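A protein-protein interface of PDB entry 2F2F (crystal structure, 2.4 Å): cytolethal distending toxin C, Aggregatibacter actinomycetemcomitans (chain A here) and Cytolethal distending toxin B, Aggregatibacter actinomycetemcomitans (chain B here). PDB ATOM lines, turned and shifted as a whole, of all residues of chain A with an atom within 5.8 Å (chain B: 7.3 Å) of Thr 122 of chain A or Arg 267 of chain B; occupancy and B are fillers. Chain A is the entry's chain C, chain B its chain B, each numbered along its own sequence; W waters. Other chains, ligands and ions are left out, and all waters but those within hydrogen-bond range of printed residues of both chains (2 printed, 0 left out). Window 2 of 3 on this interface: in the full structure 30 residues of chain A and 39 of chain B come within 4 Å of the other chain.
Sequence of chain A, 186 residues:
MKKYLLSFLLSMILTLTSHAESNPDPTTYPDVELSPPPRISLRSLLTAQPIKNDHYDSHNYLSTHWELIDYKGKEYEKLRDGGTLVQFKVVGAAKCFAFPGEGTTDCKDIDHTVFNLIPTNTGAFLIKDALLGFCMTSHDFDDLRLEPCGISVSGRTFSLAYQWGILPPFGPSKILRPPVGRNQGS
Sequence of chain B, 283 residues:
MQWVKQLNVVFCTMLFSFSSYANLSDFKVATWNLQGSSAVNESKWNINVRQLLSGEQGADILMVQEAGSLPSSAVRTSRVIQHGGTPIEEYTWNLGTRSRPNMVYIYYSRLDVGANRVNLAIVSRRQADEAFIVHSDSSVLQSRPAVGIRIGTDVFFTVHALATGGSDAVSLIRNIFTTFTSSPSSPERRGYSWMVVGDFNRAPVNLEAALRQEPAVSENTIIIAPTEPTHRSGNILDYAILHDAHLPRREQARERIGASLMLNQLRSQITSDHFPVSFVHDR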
ATOM      1  N   THR A 120     -31.069  -5.820 -23.017  1.00  0.00           N
ATOM      2  CA  THR A 120     -30.903  -5.736 -21.573  1.00  0.00           C
ATOM      3  C   THR A 120     -30.394  -4.356 -21.165  1.00  0.00           C
ATOM      4  O   THR A 120     -30.059  -3.531 -22.012  1.00  0.00           O
ATOM      5  CB  THR A 120     -29.875  -6.748 -21.004  1.00  0.00           C
ATOM      6  OG1 THR A 120     -29.363  -7.570 -22.037  1.00  0.00           O
ATOM      7  CG2 THR A 120     -30.523  -7.674 -20.060  1.00  0.00           C
ATOM      8  N   ASN A 121     -30.309  -4.133 -19.855  1.00  0.00           N
ATOM      9  CA  ASN A 121     -29.830  -2.871 -19.333  1.00  0.00           C
ATOM     10  C   ASN A 121     -28.311  -2.753 -19.383  1.00  0.00           C
ATOM     11  O   ASN A 121     -27.763  -1.686 -19.118  1.00  0.00           O
ATOM     12  CB  ASN A 121     -30.318  -2.694 -17.892  1.00  0.00           C
ATOM     13  CG  ASN A 121     -29.721  -3.718 -16.939  1.00  0.00           C
ATOM     14  OD1 ASN A 121     -29.426  -4.863 -17.319  1.00  0.00           O
ATOM     15  ND2 ASN A 121     -29.552  -3.317 -15.692  1.00  0.00           N
ATOM     16  N   THR A 122     -27.620  -3.828 -19.738  1.00  0.00           N
ATOM     17  CA  THR A 122     -26.163  -3.772 -19.805  1.00  0.00           C
ATOM     18  C   THR A 122     -25.549  -3.799 -21.201  1.00  0.00           C
ATOM     19  O   THR A 122     -24.348  -3.567 -21.356  1.00  0.00           O
ATOM     20  CB  THR A 122     -25.517  -4.908 -18.997  1.00  0.00           C
ATOM     21  OG1 THR A 122     -25.800  -6.154 -19.632  1.00  0.00           O
ATOM     22  CG2 THR A 122     -26.078  -4.928 -17.577  1.00  0.00           C
ATOM     23  N   GLY A 123     -26.347  -4.072 -22.223  1.00  0.00           N
ATOM     24  CA  GLY A 123     -25.786  -4.148 -23.565  1.00  0.00           C
ATOM     25  C   GLY A 123     -25.612  -5.600 -23.998  1.00  0.00           C
ATOM     26  O   GLY A 123     -25.265  -5.873 -25.135  1.00  0.00           O
ATOM     27  N   ALA A 124     -25.828  -6.526 -23.068  1.00  0.00           N
ATOM     28  CA  ALA A 124     -25.727  -7.961 -23.338  1.00  0.00           C
ATOM     29  C   ALA A 124     -27.057  -8.335 -23.952  1.00  0.00           C
ATOM     30  O   ALA A 124     -27.999  -7.562 -23.877  1.00  0.00           O
ATOM     31  CB  ALA A 124     -25.541  -8.743 -22.044  1.00  0.00           C
ATOM     32  N   GLN A 163     -26.478 -14.691 -21.031  1.00  0.00           N
ATOM     33  CA  GLN A 163     -26.051 -13.529 -21.796  1.00  0.00           C
ATOM     34  C   GLN A 163     -25.102 -13.752 -22.950  1.00  0.00           C
ATOM     35  O   GLN A 163     -24.140 -14.527 -22.852  1.00  0.00           O
ATOM     36  CB  GLN A 163     -25.469 -12.486 -20.843  1.00  0.00           C
ATOM     37  CG  GLN A 163     -26.424 -12.108 -19.718  1.00  0.00           C
ATOM     38  CD  GLN A 163     -25.785 -11.166 -18.731  1.00  0.00           C
ATOM     39  OE1 GLN A 163     -24.943 -10.333 -19.101  1.00  0.00           O
ATOM     40  NE2 GLN A 163     -26.167 -11.292 -17.458  1.00  0.00           N
ATOM     41  N   GLY A 165     -22.932 -11.693 -26.258  1.00  0.00           N
ATOM     42  CA  GLY A 165     -22.414 -10.428 -26.722  1.00  0.00           C
ATOM     43  C   GLY A 165     -22.324 -10.509 -28.231  1.00  0.00           C
ATOM     44  O   GLY A 165     -21.780 -11.479 -28.757  1.00  0.00           O
ATOM     45  N   ILE A 166     -22.885  -9.522 -28.924  1.00  0.00           N
ATOM     46  CA  ILE A 166     -22.823  -9.449 -30.388  1.00  0.00           C
ATOM     47  C   ILE A 166     -21.631  -8.537 -30.636  1.00  0.00           C
ATOM     48  O   ILE A 166     -21.747  -7.309 -30.599  1.00  0.00           O
ATOM     49  CB  ILE A 166     -24.125  -8.848 -30.964  1.00  0.00           C
ATOM     50  CG1 ILE A 166     -25.291  -9.777 -30.622  1.00  0.00           C
ATOM     51  CG2 ILE A 166     -24.008  -8.670 -32.464  1.00  0.00           C
ATOM     52  CD1 ILE A 166     -26.603  -9.327 -31.140  1.00  0.00           C
ATOM     53  N   LEU A 167     -20.475  -9.154 -30.870  1.00  0.00           N
ATOM     54  CA  LEU A 167     -19.233  -8.411 -31.014  1.00  0.00           C
ATOM     55  C   LEU A 167     -18.531  -8.466 -32.367  1.00  0.00           C
ATOM     56  O   LEU A 167     -18.946  -9.181 -33.260  1.00  0.00           O
ATOM     57  CB  LEU A 167     -18.272  -8.870 -29.893  1.00  0.00           C
ATOM     58  CG  LEU A 167     -18.884  -8.877 -28.477  1.00  0.00           C
ATOM     59  CD1 LEU A 167     -18.163  -9.868 -27.591  1.00  0.00           C
ATOM     60  CD2 LEU A 167     -18.803  -7.489 -27.869  1.00  0.00           C
ATOM     61  N   ILE B  47     -29.672  -2.813 -31.169  1.00  0.00           N
ATOM     62  CA  ILE B  47     -28.308  -3.105 -30.734  1.00  0.00           C
ATOM     63  C   ILE B  47     -27.552  -1.803 -30.490  1.00  0.00           C
ATOM     64  O   ILE B  47     -27.206  -1.485 -29.366  1.00  0.00           O
ATOM     65  CB  ILE B  47     -27.542  -3.948 -31.787  1.00  0.00           C
ATOM     66  CG1 ILE B  47     -28.176  -5.324 -31.939  1.00  0.00           C
ATOM     67  CG2 ILE B  47     -26.100  -4.177 -31.354  1.00  0.00           C
ATOM     68  CD1 ILE B  47     -27.447  -6.168 -32.954  1.00  0.00           C
ATOM     69  N   ASN B  48     -27.319  -1.033 -31.540  1.00  0.00           N
ATOM     70  CA  ASN B  48     -26.585   0.209 -31.409  1.00  0.00           C
ATOM     71  C   ASN B  48     -27.349   1.455 -30.949  1.00  0.00           C
ATOM     72  O   ASN B  48     -26.891   2.174 -30.070  1.00  0.00           O
ATOM     73  CB  ASN B  48     -25.862   0.516 -32.714  1.00  0.00           C
ATOM     74  CG  ASN B  48     -24.824  -0.531 -33.058  1.00  0.00           C
ATOM     75  OD1 ASN B  48     -24.830  -1.076 -34.160  1.00  0.00           O
ATOM     76  ND2 ASN B  48     -23.920  -0.817 -32.116  1.00  0.00           N
ATOM     77  N   GLN B  51     -27.979   1.602 -27.304  1.00  0.00           N
ATOM     78  CA  GLN B  51     -26.770   1.852 -26.536  1.00  0.00           C
ATOM     79  C   GLN B  51     -26.340   3.333 -26.538  1.00  0.00           C
ATOM     80  O   GLN B  51     -25.815   3.840 -25.538  1.00  0.00           O
ATOM     81  CB  GLN B  51     -25.643   0.930 -27.043  1.00  0.00           C
ATOM     82  CG  GLN B  51     -25.820  -0.510 -26.525  1.00  0.00           C
ATOM     83  CD  GLN B  51     -25.062  -1.565 -27.331  1.00  0.00           C
ATOM     84  OE1 GLN B  51     -24.040  -1.275 -27.968  1.00  0.00           O
ATOM     85  NE2 GLN B  51     -25.566  -2.807 -27.302  1.00  0.00           N
ATOM     86  N   SER B  54     -28.448   5.288 -23.902  1.00  0.00           N
ATOM     87  CA  SER B  54     -28.390   4.876 -22.498  1.00  0.00           C
ATOM     88  C   SER B  54     -27.212   5.380 -21.670  1.00  0.00           C
ATOM     89  O   SER B  54     -26.248   5.943 -22.187  1.00  0.00           O
ATOM     90  CB  SER B  54     -28.413   3.351 -22.415  1.00  0.00           C
ATOM     91  OG  SER B  54     -27.105   2.857 -22.623  1.00  0.00           O
ATOM     92  N   GLY B  55     -27.304   5.136 -20.366  1.00  0.00           N
ATOM     93  CA  GLY B  55     -26.252   5.534 -19.456  1.00  0.00           C
ATOM     94  C   GLY B  55     -26.203   7.011 -19.128  1.00  0.00           C
ATOM     95  O   GLY B  55     -27.007   7.814 -19.596  1.00  0.00           O
ATOM     96  N   GLN B  57     -23.984   8.994 -20.041  1.00  0.00           N
ATOM     97  CA  GLN B  57     -23.533   9.725 -21.218  1.00  0.00           C
ATOM     98  C   GLN B  57     -24.402   9.525 -22.452  1.00  0.00           C
ATOM     99  O   GLN B  57     -23.982   9.858 -23.556  1.00  0.00           O
ATOM    100  CB  GLN B  57     -22.088   9.370 -21.533  1.00  0.00           C
ATOM    101  CG  GLN B  57     -21.128   9.967 -20.542  1.00  0.00           C
ATOM    102  CD  GLN B  57     -19.869   9.165 -20.397  1.00  0.00           C
ATOM    103  OE1 GLN B  57     -18.939   9.310 -21.196  1.00  0.00           O
ATOM    104  NE2 GLN B  57     -19.818   8.306 -19.367  1.00  0.00           N
ATOM    105  N   LEU B 263     -17.556   5.862 -29.071  1.00  0.00           N
ATOM    106  CA  LEU B 263     -17.294   4.459 -28.795  1.00  0.00           C
ATOM    107  C   LEU B 263     -17.420   4.106 -27.319  1.00  0.00           C
ATOM    108  O   LEU B 263     -17.539   2.942 -26.975  1.00  0.00           O
ATOM    109  CB  LEU B 263     -15.912   4.079 -29.313  1.00  0.00           C
ATOM    110  CG  LEU B 263     -15.581   4.487 -30.754  1.00  0.00           C
ATOM    111  CD1 LEU B 263     -14.153   4.110 -31.045  1.00  0.00           C
ATOM    112  CD2 LEU B 263     -16.509   3.820 -31.746  1.00  0.00           C
ATOM    113  N   ASN B 264     -17.444   5.112 -26.454  1.00  0.00           N
ATOM    114  CA  ASN B 264     -17.571   4.877 -25.016  1.00  0.00           C
ATOM    115  C   ASN B 264     -18.948   4.375 -24.663  1.00  0.00           C
ATOM    116  O   ASN B 264     -19.194   3.960 -23.526  1.00  0.00           O
ATOM    117  CB  ASN B 264     -17.288   6.162 -24.237  1.00  0.00           C
ATOM    118  CG  ASN B 264     -18.249   7.290 -24.592  1.00  0.00           C
ATOM    119  OD1 ASN B 264     -18.171   7.861 -25.675  1.00  0.00           O
ATOM    120  ND2 ASN B 264     -19.158   7.607 -23.680  1.00  0.00           N
ATOM    121  N   GLN B 265     -19.860   4.433 -25.629  1.00  0.00           N
ATOM    122  CA  GLN B 265     -21.243   4.000 -25.415  1.00  0.00           C
ATOM    123  C   GLN B 265     -21.526   2.571 -25.896  1.00  0.00           C
ATOM    124  O   GLN B 265     -22.577   2.008 -25.597  1.00  0.00           O
ATOM    125  CB  GLN B 265     -22.199   4.945 -26.155  1.00  0.00           C
ATOM    126  CG  GLN B 265     -22.400   6.307 -25.522  1.00  0.00           C
ATOM    127  CD  GLN B 265     -23.038   6.223 -24.170  1.00  0.00           C
ATOM    128  OE1 GLN B 265     -22.363   6.342 -23.156  1.00  0.00           O
ATOM    129  NE2 GLN B 265     -24.350   6.018 -24.141  1.00  0.00           N
ATOM    130  N   LEU B 266     -20.608   1.991 -26.655  1.00  0.00           N
ATOM    131  CA  LEU B 266     -20.837   0.654 -27.191  1.00  0.00           C
ATOM    132  C   LEU B 266     -20.540  -0.558 -26.308  1.00  0.00           C
ATOM    133  O   LEU B 266     -19.575  -0.585 -25.557  1.00  0.00           O
ATOM    134  CB  LEU B 266     -20.069   0.496 -28.507  1.00  0.00           C
ATOM    135  CG  LEU B 266     -20.061   1.686 -29.467  1.00  0.00           C
ATOM    136  CD1 LEU B 266     -19.123   1.389 -30.605  1.00  0.00           C
ATOM    137  CD2 LEU B 266     -21.451   1.975 -29.991  1.00  0.00           C
ATOM    138  N   ARG B 267     -21.397  -1.562 -26.450  1.00  0.00           N
ATOM    139  CA  ARG B 267     -21.301  -2.845 -25.768  1.00  0.00           C
ATOM    140  C   ARG B 267     -21.402  -3.960 -26.834  1.00  0.00           C
ATOM    141  O   ARG B 267     -21.570  -5.137 -26.514  1.00  0.00           O
ATOM    142  CB  ARG B 267     -22.437  -2.991 -24.763  1.00  0.00           C
ATOM    143  CG  ARG B 267     -22.665  -1.760 -23.925  1.00  0.00           C
ATOM    144  CD  ARG B 267     -21.501  -1.454 -23.006  1.00  0.00           C
ATOM    145  NE  ARG B 267     -21.827  -0.386 -22.062  1.00  0.00           N
ATOM    146  CZ  ARG B 267     -21.165   0.767 -21.974  1.00  0.00           C
ATOM    147  NH1 ARG B 267     -20.134   1.020 -22.772  1.00  0.00           N
ATOM    148  NH2 ARG B 267     -21.525   1.672 -21.074  1.00  0.00           N
ATOM    149  N   SER B 268     -21.393  -3.548 -28.098  1.00  0.00           N
ATOM    150  CA  SER B 268     -21.502  -4.466 -29.220  1.00  0.00           C
ATOM    151  C   SER B 268     -20.784  -3.976 -30.443  1.00  0.00           C
ATOM    152  O   SER B 268     -20.229  -2.882 -30.474  1.00  0.00           O
ATOM    153  CB  SER B 268     -22.954  -4.666 -29.663  1.00  0.00           C
ATOM    154  OG  SER B 268     -23.877  -4.489 -28.611  1.00  0.00           O
ATOM    155  N   GLN B 269     -20.815  -4.820 -31.464  1.00  0.00           N
ATOM    156  CA  GLN B 269     -20.228  -4.497 -32.742  1.00  0.00           C
ATOM    157  C   GLN B 269     -21.041  -3.307 -33.268  1.00  0.00           C
ATOM    158  O   GLN B 269     -22.236  -3.224 -33.008  1.00  0.00           O
ATOM    159  CB  GLN B 269     -20.415  -5.697 -33.680  1.00  0.00           C
ATOM    160  CG  GLN B 269     -20.277  -5.422 -35.146  1.00  0.00           C
ATOM    161  CD  GLN B 269     -18.889  -5.017 -35.472  1.00  0.00           C
ATOM    162  OE1 GLN B 269     -18.327  -4.164 -34.798  1.00  0.00           O
ATOM    163  NE2 GLN B 269     -18.308  -5.619 -36.495  1.00  0.00           N
HETATM  164  O   HOH W   1     -23.246  -1.453 -19.963  1.00  0.00           O
HETATM  165  O   HOH W   2     -23.456  -7.204 -26.930  1.00  0.00           O
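The backbone NH of Gln 269 of chain B sits at hydrogen-bond distance from the backbone carbonyl oxygen of Ile 166 of chain A, at 2.8 Å.
The backbone carbonyl oxygen (O) of Ile 47 of chain B sits at hydrogen-bond distance from the side-chain amide nitrogen (NE2) of Gln 51 of chain B.
The backbone carbonyl oxygen (O) of Gln 269 of chain B is in hydrogen-bond range of the side-chain amide nitrogen (ND2) of Asn 48 of chain B (3.1 Å).
The backbone carbonyl oxygen (O) of Asn 264 of chain B sits at hydrogen-bond distance from the guanidinium group (NH1) of Arg 267 of chain B (3.2 Å).
The side-chain amide nitrogen (NE2) of Gln 265 of chain B is in hydrogen-bond range of the backbone carbonyl oxygen (O) of Gln 51 of chain B (3.0 Å).
NE2 of Gln 51 of chain B is in hydrogen-bond range of OG of Ser 268 of chain B, at 2.7 Å.
The side-chain hydroxyl (OG) of Ser 54 of chain B lies within hydrogen-bond range of the backbone carbonyl oxygen (O) of Gln 51 of chain B, at 3.3 Å.
Printed residues of chain B that touch a printed residue of chain A: Ile 47, Gln 51, Arg 267, Ser 268 and Gln 269.
Of the 9 printed residues of chain A, 4 touch a printed residue of chain B.
Hydrophobic or aromatic side chains of chain A within 4 Å of the printed part of chain B: Ile 166 and Leu 167.
Among the printed residues, 9 pairs touch across the chains.
Among the printed residues, no Asp or Glu carboxylate lies within 4 Å of a Lys or Arg side-chain nitrogen of the other chain.
Among the printed residues, pairs that only touch across the chains: Thr 122 of chain A with Arg 267 of chain B (3.6 Å), Gly 123 of chain A with Gln 51 of chain B (3.8 Å), Gly 123 of chain A with Arg 267 of chain B (3.7 Å), Gly 123 of chain A with Ser 268 of chain B (3.99 Å), Ile 166 of chain A with Ile 47 of chain B (3.7 Å), Ile 166 of chain A with Ser 268 of chain B (3.1 Å), Leu 167 of chain A with Arg 267 of chain B (3.9 Å) and Leu 167 of chain A with Gln 269 of chain B (3.6 Å).
Of chain B, only Arg 267 comes within 4 Å of Thr 122 of chain A.
Of the printed residues of chain B, Ile 166 of chain A touches Ile 47, Ser 268 and Gln 269.
Gln 265 of chain B touches none of the printed residues of chain A.
Of the printed residues of chain A, Gln 269 of chain B touches Ile 166 (2.8 Å) and Leu 167 (3.6 Å).
The nearest residue of chain B that does not touch Thr 122 of chain A is Gln 51 of chain B (6.1 Å).
Water W1 lies within hydrogen-bond range of NE of Arg 267 of chain B (2.7 Å) and O of Thr 122 of chain A (2.8 Å).
Water W2 lies within hydrogen-bond range of the backbone carbonyl oxygen of Arg 267 of chain B, the backbone carbonyl oxygen of Gly 123 of chain A, the backbone NH of Ile 166 of chain A and the side-chain hydroxyl of Ser 268 of chain B.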
